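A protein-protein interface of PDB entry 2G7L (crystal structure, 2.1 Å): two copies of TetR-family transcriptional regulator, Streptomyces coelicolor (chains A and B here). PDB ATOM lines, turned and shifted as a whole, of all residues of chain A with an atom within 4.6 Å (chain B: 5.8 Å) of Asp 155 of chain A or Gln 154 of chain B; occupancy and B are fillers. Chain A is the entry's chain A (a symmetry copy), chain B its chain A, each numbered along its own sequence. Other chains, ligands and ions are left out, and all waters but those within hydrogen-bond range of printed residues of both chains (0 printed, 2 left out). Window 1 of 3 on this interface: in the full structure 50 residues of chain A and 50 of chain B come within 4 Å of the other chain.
The side-chain amide oxygen (OE1) of Gln 154 of chain B sits at hydrogen-bond distance from the side-chain hydroxyl (OG1) of Thr 159 of chain A (3.5 Å).
The side-chain amide oxygen (OE1) of Gln 154 of chain B sits close to the side-chain carboxylate (OE2) of Glu 162 of chain A, at 3.1 Å.
The side-chain amide oxygen (OE1) of Gln 154 of chain A sits at hydrogen-bond distance from the side-chain hydroxyl (OG1) of Thr 159 of chain B (3.5 Å).
OG1 of Thr 159 of chain A is in hydrogen-bond range of O of Asp 155 of chain A.
O of Asp 155 of chain B lies within hydrogen-bond range of OG1 of Thr 159 of chain B (3.1 Å).
OD2 of Asp 155 of chain A is in hydrogen-bond range of OG of Ser 213 of chain A, 3.1 Å away.
Among the printed residues, merely in contact across the chains: Glu 162 of chain A with Leu 115 of chain B (3.0 Å), Gln 154 of chain A with Ala 158 of chain B (3.5 Å), Ala 158 of chain A with Gln 154 of chain B (3.5 Å), Ala 158 of chain A with Ala 158 of chain B (3.6 Å), Asp 155 of chain A with Gln 154 of chain B (3.7 Å) and Gln 154 of chain A with Asp 155 of chain B (3.7 Å).
Leu 153 of chain A touches none of the printed residues of chain B.
Printed residues of chain B within 4 Å of Gln 154 of chain A: Asp 155 (3.7 Å), Ala 158 (3.5 Å) and Thr 159 (3.5 Å).
Asp 155 of chain A touches just one residue of chain B: Gln 154.
Of the printed residues of chain B, Ala 158 of chain A touches Gln 154 (3.5 Å) and Ala 158 (3.6 Å).
Of the printed residues of chain A, Leu 115 of chain B touches Glu 162 (3.0 Å).
Lys 151 of chain B touches none of the printed residues of chain A.
Of chain A, only Asp 155 (3.7 Å), Ala 158 (3.5 Å), Thr 159 (3.5 Å) and Glu 162 (3.1 Å) come within 4 Å of Gln 154 of chain B.
Printed residues of chain A within 4 Å of Asp 155 of chain B: Gln 154 (3.7 Å).
Printed residues of chain B that touch a printed residue of chain A: Leu 115, Gln 154, Asp 155, Ala 158 and Thr 159.
Hydrophobic or aromatic side chains of chain B within 4 Å of the printed part of chain A: Ala 158.
Of the 12 printed residues of chain A, 5 touch a printed residue of chain B.
Printed residues of chain A that touch a printed residue of chain B: Gln 154, Asp 155, Ala 158, Thr 159 and Glu 162.
Hydrophobic or aromatic side chains of chain A within 4 Å of the printed part of chain B: Ala 158.
Among the printed residues, no Asp or Glu carboxylate lies within 4 Å of a Lys or Arg side-chain nitrogen of the other chain.
Gln 154 of chain A touches Asp 155 of chain B, and with the chains exchanged Asp 155 of chain A touches Gln 154 of chain B.
Gln 154 of chain A touches Ala 158 of chain B, and with the chains exchanged Ala 158 of chain A touches Gln 154 of chain B.
Gln 154 of chain A touches Thr 159 of chain B, and with the chains exchanged Thr 159 of chain A touches Gln 154 of chain B.
Ala 158 of chain A touches its own counterpart, Ala 158 of chain B.
Positions printed for both chains: 151, 152, 153, 154, 155, 156, 157, 158 and 159.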
ATOM      1  N   LYS A 151     -21.567 -18.300   0.538  1.00  0.00           N
ATOM      2  CA  LYS A 151     -22.101 -19.199   1.566  1.00  0.00           C
ATOM      3  C   LYS A 151     -23.579 -19.364   1.500  1.00  0.00           C
ATOM      4  O   LYS A 151     -24.062 -20.474   1.648  1.00  0.00           O
ATOM      5  CB  LYS A 151     -21.702 -18.721   2.991  1.00  0.00           C
ATOM      6  CG  LYS A 151     -20.287 -19.203   3.326  1.00  0.00           C
ATOM      7  CD  LYS A 151     -19.182 -18.141   3.287  1.00  0.00           C
ATOM      8  CE  LYS A 151     -17.721 -18.662   2.726  1.00  0.00           C
ATOM      9  NZ  LYS A 151     -17.504 -17.957   1.351  1.00  0.00           N
ATOM     10  N   LEU A 152     -24.336 -18.272   1.312  1.00  0.00           N
ATOM     11  CA  LEU A 152     -25.817 -18.401   1.111  1.00  0.00           C
ATOM     12  C   LEU A 152     -26.189 -19.222  -0.144  1.00  0.00           C
ATOM     13  O   LEU A 152     -27.151 -19.995  -0.169  1.00  0.00           O
ATOM     14  CB  LEU A 152     -26.436 -17.012   1.022  1.00  0.00           C
ATOM     15  CG  LEU A 152     -26.540 -16.155   2.275  1.00  0.00           C
ATOM     16  CD1 LEU A 152     -26.707 -14.700   1.879  1.00  0.00           C
ATOM     17  CD2 LEU A 152     -27.665 -16.743   3.253  1.00  0.00           C
ATOM     18  N   LEU A 153     -25.396 -19.085  -1.201  1.00  0.00           N
ATOM     19  CA  LEU A 153     -25.685 -19.847  -2.424  1.00  0.00           C
ATOM     20  C   LEU A 153     -25.300 -21.321  -2.243  1.00  0.00           C
ATOM     21  O   LEU A 153     -26.077 -22.227  -2.605  1.00  0.00           O
ATOM     22  CB  LEU A 153     -24.960 -19.213  -3.654  1.00  0.00           C
ATOM     23  CG  LEU A 153     -25.617 -17.895  -4.179  1.00  0.00           C
ATOM     24  CD1 LEU A 153     -24.780 -17.160  -5.225  1.00  0.00           C
ATOM     25  CD2 LEU A 153     -27.000 -18.166  -4.659  1.00  0.00           C
ATOM     26  N   GLN A 154     -24.088 -21.542  -1.732  1.00  0.00           N
ATOM     27  CA  GLN A 154     -23.615 -22.907  -1.493  1.00  0.00           C
ATOM     28  C   GLN A 154     -24.549 -23.686  -0.572  1.00  0.00           C
ATOM     29  O   GLN A 154     -24.742 -24.852  -0.741  1.00  0.00           O
ATOM     30  CB  GLN A 154     -22.229 -22.920  -0.892  1.00  0.00           C
ATOM     31  CG  GLN A 154     -21.626 -24.364  -0.938  1.00  0.00           C
ATOM     32  CD  GLN A 154     -20.471 -24.462  -0.048  1.00  0.00           C
ATOM     33  OE1 GLN A 154     -19.346 -24.302  -0.470  1.00  0.00           O
ATOM     34  NE2 GLN A 154     -20.736 -24.648   1.237  1.00  0.00           N
ATOM     35  N   ASP A 155     -25.115 -23.015   0.407  1.00  0.00           N
ATOM     36  CA  ASP A 155     -26.010 -23.627   1.395  1.00  0.00           C
ATOM     37  C   ASP A 155     -27.313 -24.092   0.739  1.00  0.00           C
ATOM     38  O   ASP A 155     -27.780 -25.217   1.005  1.00  0.00           O
ATOM     39  CB  ASP A 155     -26.271 -22.606   2.508  1.00  0.00           C
ATOM     40  CG  ASP A 155     -27.372 -23.055   3.500  1.00  0.00           C
ATOM     41  OD1 ASP A 155     -27.185 -24.132   4.163  1.00  0.00           O
ATOM     42  OD2 ASP A 155     -28.398 -22.323   3.609  1.00  0.00           O
ATOM     43  N   ALA A 156     -27.922 -23.257  -0.110  1.00  0.00           N
ATOM     44  CA  ALA A 156     -29.151 -23.672  -0.788  1.00  0.00           C
ATOM     45  C   ALA A 156     -28.859 -24.826  -1.735  1.00  0.00           C
ATOM     46  O   ALA A 156     -29.590 -25.814  -1.797  1.00  0.00           O
ATOM     47  CB  ALA A 156     -29.799 -22.471  -1.568  1.00  0.00           C
ATOM     48  N   THR A 157     -27.741 -24.707  -2.442  1.00  0.00           N
ATOM     49  CA  THR A 157     -27.308 -25.715  -3.389  1.00  0.00           C
ATOM     50  C   THR A 157     -27.033 -27.025  -2.708  1.00  0.00           C
ATOM     51  O   THR A 157     -27.433 -28.055  -3.219  1.00  0.00           O
ATOM     52  CB  THR A 157     -26.002 -25.293  -4.089  1.00  0.00           C
ATOM     53  OG1 THR A 157     -26.137 -23.953  -4.604  1.00  0.00           O
ATOM     54  CG2 THR A 157     -25.652 -26.233  -5.220  1.00  0.00           C
ATOM     55  N   ALA A 158     -26.293 -27.010  -1.575  1.00  0.00           N
ATOM     56  CA  ALA A 158     -26.036 -28.271  -0.818  1.00  0.00           C
ATOM     57  C   ALA A 158     -27.335 -28.890  -0.359  1.00  0.00           C
ATOM     58  O   ALA A 158     -27.498 -30.094  -0.464  1.00  0.00           O
ATOM     59  CB  ALA A 158     -25.072 -28.048   0.354  1.00  0.00           C
ATOM     60  N   THR A 159     -28.276 -28.094   0.094  1.00  0.00           N
ATOM     61  CA  THR A 159     -29.568 -28.644   0.577  1.00  0.00           C
ATOM     62  C   THR A 159     -30.447 -29.227  -0.540  1.00  0.00           C
ATOM     63  O   THR A 159     -31.180 -30.215  -0.345  1.00  0.00           O
ATOM     64  CB  THR A 159     -30.397 -27.605   1.397  1.00  0.00           C
ATOM     65  OG1 THR A 159     -29.651 -27.171   2.551  1.00  0.00           O
ATOM     66  CG2 THR A 159     -31.720 -28.226   1.920  1.00  0.00           C
ATOM     67  N   GLU A 162     -29.262 -32.817  -1.736  1.00  0.00           N
ATOM     68  CA  GLU A 162     -29.758 -33.902  -0.881  1.00  0.00           C
ATOM     69  C   GLU A 162     -31.168 -34.341  -1.226  1.00  0.00           C
ATOM     70  O   GLU A 162     -31.643 -35.308  -0.656  1.00  0.00           O
ATOM     71  CB  GLU A 162     -29.745 -33.465   0.596  1.00  0.00           C
ATOM     72  CG  GLU A 162     -28.336 -33.068   1.225  1.00  0.00           C
ATOM     73  CD  GLU A 162     -28.436 -32.689   2.743  1.00  0.00           C
ATOM     74  OE1 GLU A 162     -27.548 -33.127   3.522  1.00  0.00           O
ATOM     75  OE2 GLU A 162     -29.385 -31.956   3.166  1.00  0.00           O
ATOM     76  N   SER A 213     -31.657 -22.152   8.388  1.00  0.00           N
ATOM     77  CA  SER A 213     -30.244 -21.807   8.099  1.00  0.00           C
ATOM     78  C   SER A 213     -30.025 -20.455   7.385  1.00  0.00           C
ATOM     79  O   SER A 213     -28.925 -19.817   7.445  1.00  0.00           O
ATOM     80  CB  SER A 213     -29.534 -22.931   7.368  1.00  0.00           C
ATOM     81  OG  SER A 213     -30.075 -23.081   6.110  1.00  0.00           O
ATOM     82  N   LEU A 217     -27.313 -18.166   8.835  1.00  0.00           N
ATOM     83  CA  LEU A 217     -26.226 -17.683   7.997  1.00  0.00           C
ATOM     84  C   LEU A 217     -26.204 -16.176   7.982  1.00  0.00           C
ATOM     85  O   LEU A 217     -25.134 -15.558   8.109  1.00  0.00           O
ATOM     86  CB  LEU A 217     -26.404 -18.247   6.559  1.00  0.00           C
ATOM     87  CG  LEU A 217     -25.840 -19.687   6.472  1.00  0.00           C
ATOM     88  CD1 LEU A 217     -26.390 -20.323   5.268  1.00  0.00           C
ATOM     89  CD2 LEU A 217     -24.288 -19.584   6.345  1.00  0.00           C
ATOM     90  N   LEU B 115     -23.663 -35.961   0.213  1.00  0.00           N
ATOM     91  CA  LEU B 115     -24.877 -35.112   0.078  1.00  0.00           C
ATOM     92  C   LEU B 115     -26.072 -35.866  -0.424  1.00  0.00           C
ATOM     93  O   LEU B 115     -27.182 -35.542  -0.077  1.00  0.00           O
ATOM     94  CB  LEU B 115     -24.626 -33.845  -0.768  1.00  0.00           C
ATOM     95  CG  LEU B 115     -23.496 -32.962  -0.240  1.00  0.00           C
ATOM     96  CD1 LEU B 115     -22.827 -32.149  -1.329  1.00  0.00           C
ATOM     97  CD2 LEU B 115     -23.870 -32.084   0.960  1.00  0.00           C
ATOM     98  N   VAL B 149     -25.402 -29.085  14.244  1.00  0.00           N
ATOM     99  CA  VAL B 149     -24.346 -30.029  13.843  1.00  0.00           C
ATOM    100  C   VAL B 149     -24.616 -30.561  12.401  1.00  0.00           C
ATOM    101  O   VAL B 149     -23.684 -30.778  11.713  1.00  0.00           O
ATOM    102  CB  VAL B 149     -24.224 -31.258  14.854  1.00  0.00           C
ATOM    103  CG1 VAL B 149     -23.724 -30.757  16.280  1.00  0.00           C
ATOM    104  CG2 VAL B 149     -25.555 -31.879  15.015  1.00  0.00           C
ATOM    105  N   ASP B 150     -25.871 -30.815  12.017  1.00  0.00           N
ATOM    106  CA  ASP B 150     -26.246 -31.060  10.609  1.00  0.00           C
ATOM    107  C   ASP B 150     -25.684 -29.988   9.657  1.00  0.00           C
ATOM    108  O   ASP B 150     -25.003 -30.291   8.651  1.00  0.00           O
ATOM    109  CB  ASP B 150     -27.775 -31.086  10.531  1.00  0.00           C
ATOM    110  CG  ASP B 150     -28.355 -32.508  10.716  1.00  0.00           C
ATOM    111  OD1 ASP B 150     -27.734 -33.327  11.462  1.00  0.00           O
ATOM    112  OD2 ASP B 150     -29.427 -32.817  10.097  1.00  0.00           O
ATOM    113  N   LYS B 151     -25.866 -28.711  10.018  1.00  0.00           N
ATOM    114  CA  LYS B 151     -25.353 -27.589   9.225  1.00  0.00           C
ATOM    115  C   LYS B 151     -23.866 -27.517   9.192  1.00  0.00           C
ATOM    116  O   LYS B 151     -23.305 -27.263   8.140  1.00  0.00           O
ATOM    117  CB  LYS B 151     -25.920 -26.234   9.736  1.00  0.00           C
ATOM    118  CG  LYS B 151     -27.314 -25.996   9.144  1.00  0.00           C
ATOM    119  CD  LYS B 151     -28.497 -26.193  10.097  1.00  0.00           C
ATOM    120  CE  LYS B 151     -29.851 -26.846   9.417  1.00  0.00           C
ATOM    121  NZ  LYS B 151     -30.001 -28.275  10.028  1.00  0.00           N
ATOM    122  N   LEU B 152     -23.193 -27.703  10.338  1.00  0.00           N
ATOM    123  CA  LEU B 152     -21.694 -27.767  10.335  1.00  0.00           C
ATOM    124  C   LEU B 152     -21.139 -28.935   9.489  1.00  0.00           C
ATOM    125  O   LEU B 152     -20.115 -28.831   8.807  1.00  0.00           O
ATOM    126  CB  LEU B 152     -21.192 -27.884  11.768  1.00  0.00           C
ATOM    127  CG  LEU B 152     -21.278 -26.678  12.694  1.00  0.00           C
ATOM    128  CD1 LEU B 152     -21.201 -27.143  14.136  1.00  0.00           C
ATOM    129  CD2 LEU B 152     -20.200 -25.574  12.262  1.00  0.00           C
ATOM    130  N   LEU B 153     -21.840 -30.063   9.499  1.00  0.00           N
ATOM    131  CA  LEU B 153     -21.376 -31.209   8.705  1.00  0.00           C
ATOM    132  C   LEU B 153     -21.647 -30.976   7.214  1.00  0.00           C
ATOM    133  O   LEU B 153     -20.765 -31.216   6.366  1.00  0.00           O
ATOM    134  CB  LEU B 153     -22.038 -32.533   9.207  1.00  0.00           C
ATOM    135  CG  LEU B 153     -21.452 -33.075  10.552  1.00  0.00           C
ATOM    136  CD1 LEU B 153     -22.250 -34.231  11.153  1.00  0.00           C
ATOM    137  CD2 LEU B 153     -20.013 -33.417  10.384  1.00  0.00           C
ATOM    138  N   GLN B 154     -22.877 -30.560   6.909  1.00  0.00           N
ATOM    139  CA  GLN B 154     -23.250 -30.283   5.520  1.00  0.00           C
ATOM    140  C   GLN B 154     -22.340 -29.240   4.878  1.00  0.00           C
ATOM    141  O   GLN B 154     -22.032 -29.324   3.727  1.00  0.00           O
ATOM    142  CB  GLN B 154     -24.678 -29.805   5.411  1.00  0.00           C
ATOM    143  CG  GLN B 154     -25.147 -29.818   3.917  1.00  0.00           C
ATOM    144  CD  GLN B 154     -26.367 -29.027   3.759  1.00  0.00           C
ATOM    145  OE1 GLN B 154     -27.458 -29.553   3.794  1.00  0.00           O
ATOM    146  NE2 GLN B 154     -26.205 -27.715   3.664  1.00  0.00           N
ATOM    147  N   ASP B 155     -21.926 -28.257   5.646  1.00  0.00           N
ATOM    148  CA  ASP B 155     -21.076 -27.161   5.170  1.00  0.00           C
ATOM    149  C   ASP B 155     -19.683 -27.673   4.794  1.00  0.00           C
ATOM    150  O   ASP B 155     -19.147 -27.302   3.730  1.00  0.00           O
ATOM    151  CB  ASP B 155     -21.008 -26.092   6.266  1.00  0.00           C
ATOM    152  CG  ASP B 155     -19.967 -24.984   5.970  1.00  0.00           C
ATOM    153  OD1 ASP B 155     -20.120 -24.277   4.916  1.00  0.00           O
ATOM    154  OD2 ASP B 155     -19.022 -24.829   6.797  1.00  0.00           O
ATOM    155  N   ALA B 156     -19.073 -28.514   5.637  1.00  0.00           N
ATOM    156  CA  ALA B 156     -17.756 -29.058   5.302  1.00  0.00           C
ATOM    157  C   ALA B 156     -17.859 -29.957   4.079  1.00  0.00           C
ATOM    158  O   ALA B 156     -17.043 -29.897   3.160  1.00  0.00           O
ATOM    159  CB  ALA B 156     -17.146 -29.848   6.515  1.00  0.00           C
ATOM    160  N   THR B 157     -18.914 -30.764   4.059  1.00  0.00           N
ATOM    161  CA  THR B 157     -19.170 -31.684   2.970  1.00  0.00           C
ATOM    162  C   THR B 157     -19.391 -30.953   1.676  1.00  0.00           C
ATOM    163  O   THR B 157     -18.859 -31.367   0.662  1.00  0.00           O
ATOM    164  CB  THR B 157     -20.438 -32.518   3.234  1.00  0.00           C
ATOM    165  OG1 THR B 157     -20.373 -33.097   4.553  1.00  0.00           O
ATOM    166  CG2 THR B 157     -20.600 -33.618   2.209  1.00  0.00           C
ATOM    167  N   ALA B 158     -20.231 -29.892   1.680  1.00  0.00           N
ATOM    168  CA  ALA B 158     -20.446 -29.087   0.441  1.00  0.00           C
ATOM    169  C   ALA B 158     -19.145 -28.482  -0.032  1.00  0.00           C
ATOM    170  O   ALA B 158     -18.870 -28.501  -1.220  1.00  0.00           O
ATOM    171  CB  ALA B 158     -21.529 -28.018   0.634  1.00  0.00           C
ATOM    172  N   THR B 159     -18.323 -27.996   0.869  1.00  0.00           N
ATOM    173  CA  THR B 159     -17.037 -27.372   0.464  1.00  0.00           C
ATOM    174  C   THR B 159     -16.012 -28.373  -0.092  1.00  0.00           C
ATOM    175  O   THR B 159     -15.218 -28.058  -0.997  1.00  0.00           O
ATOM    176  CB  THR B 159     -16.379 -26.546   1.615  1.00  0.00           C
ATOM    177  OG1 THR B 159     -17.263 -25.488   2.036  1.00  0.00           O
ATOM    178  CG2 THR B 159     -15.061 -25.874   1.145  1.00  0.00           C
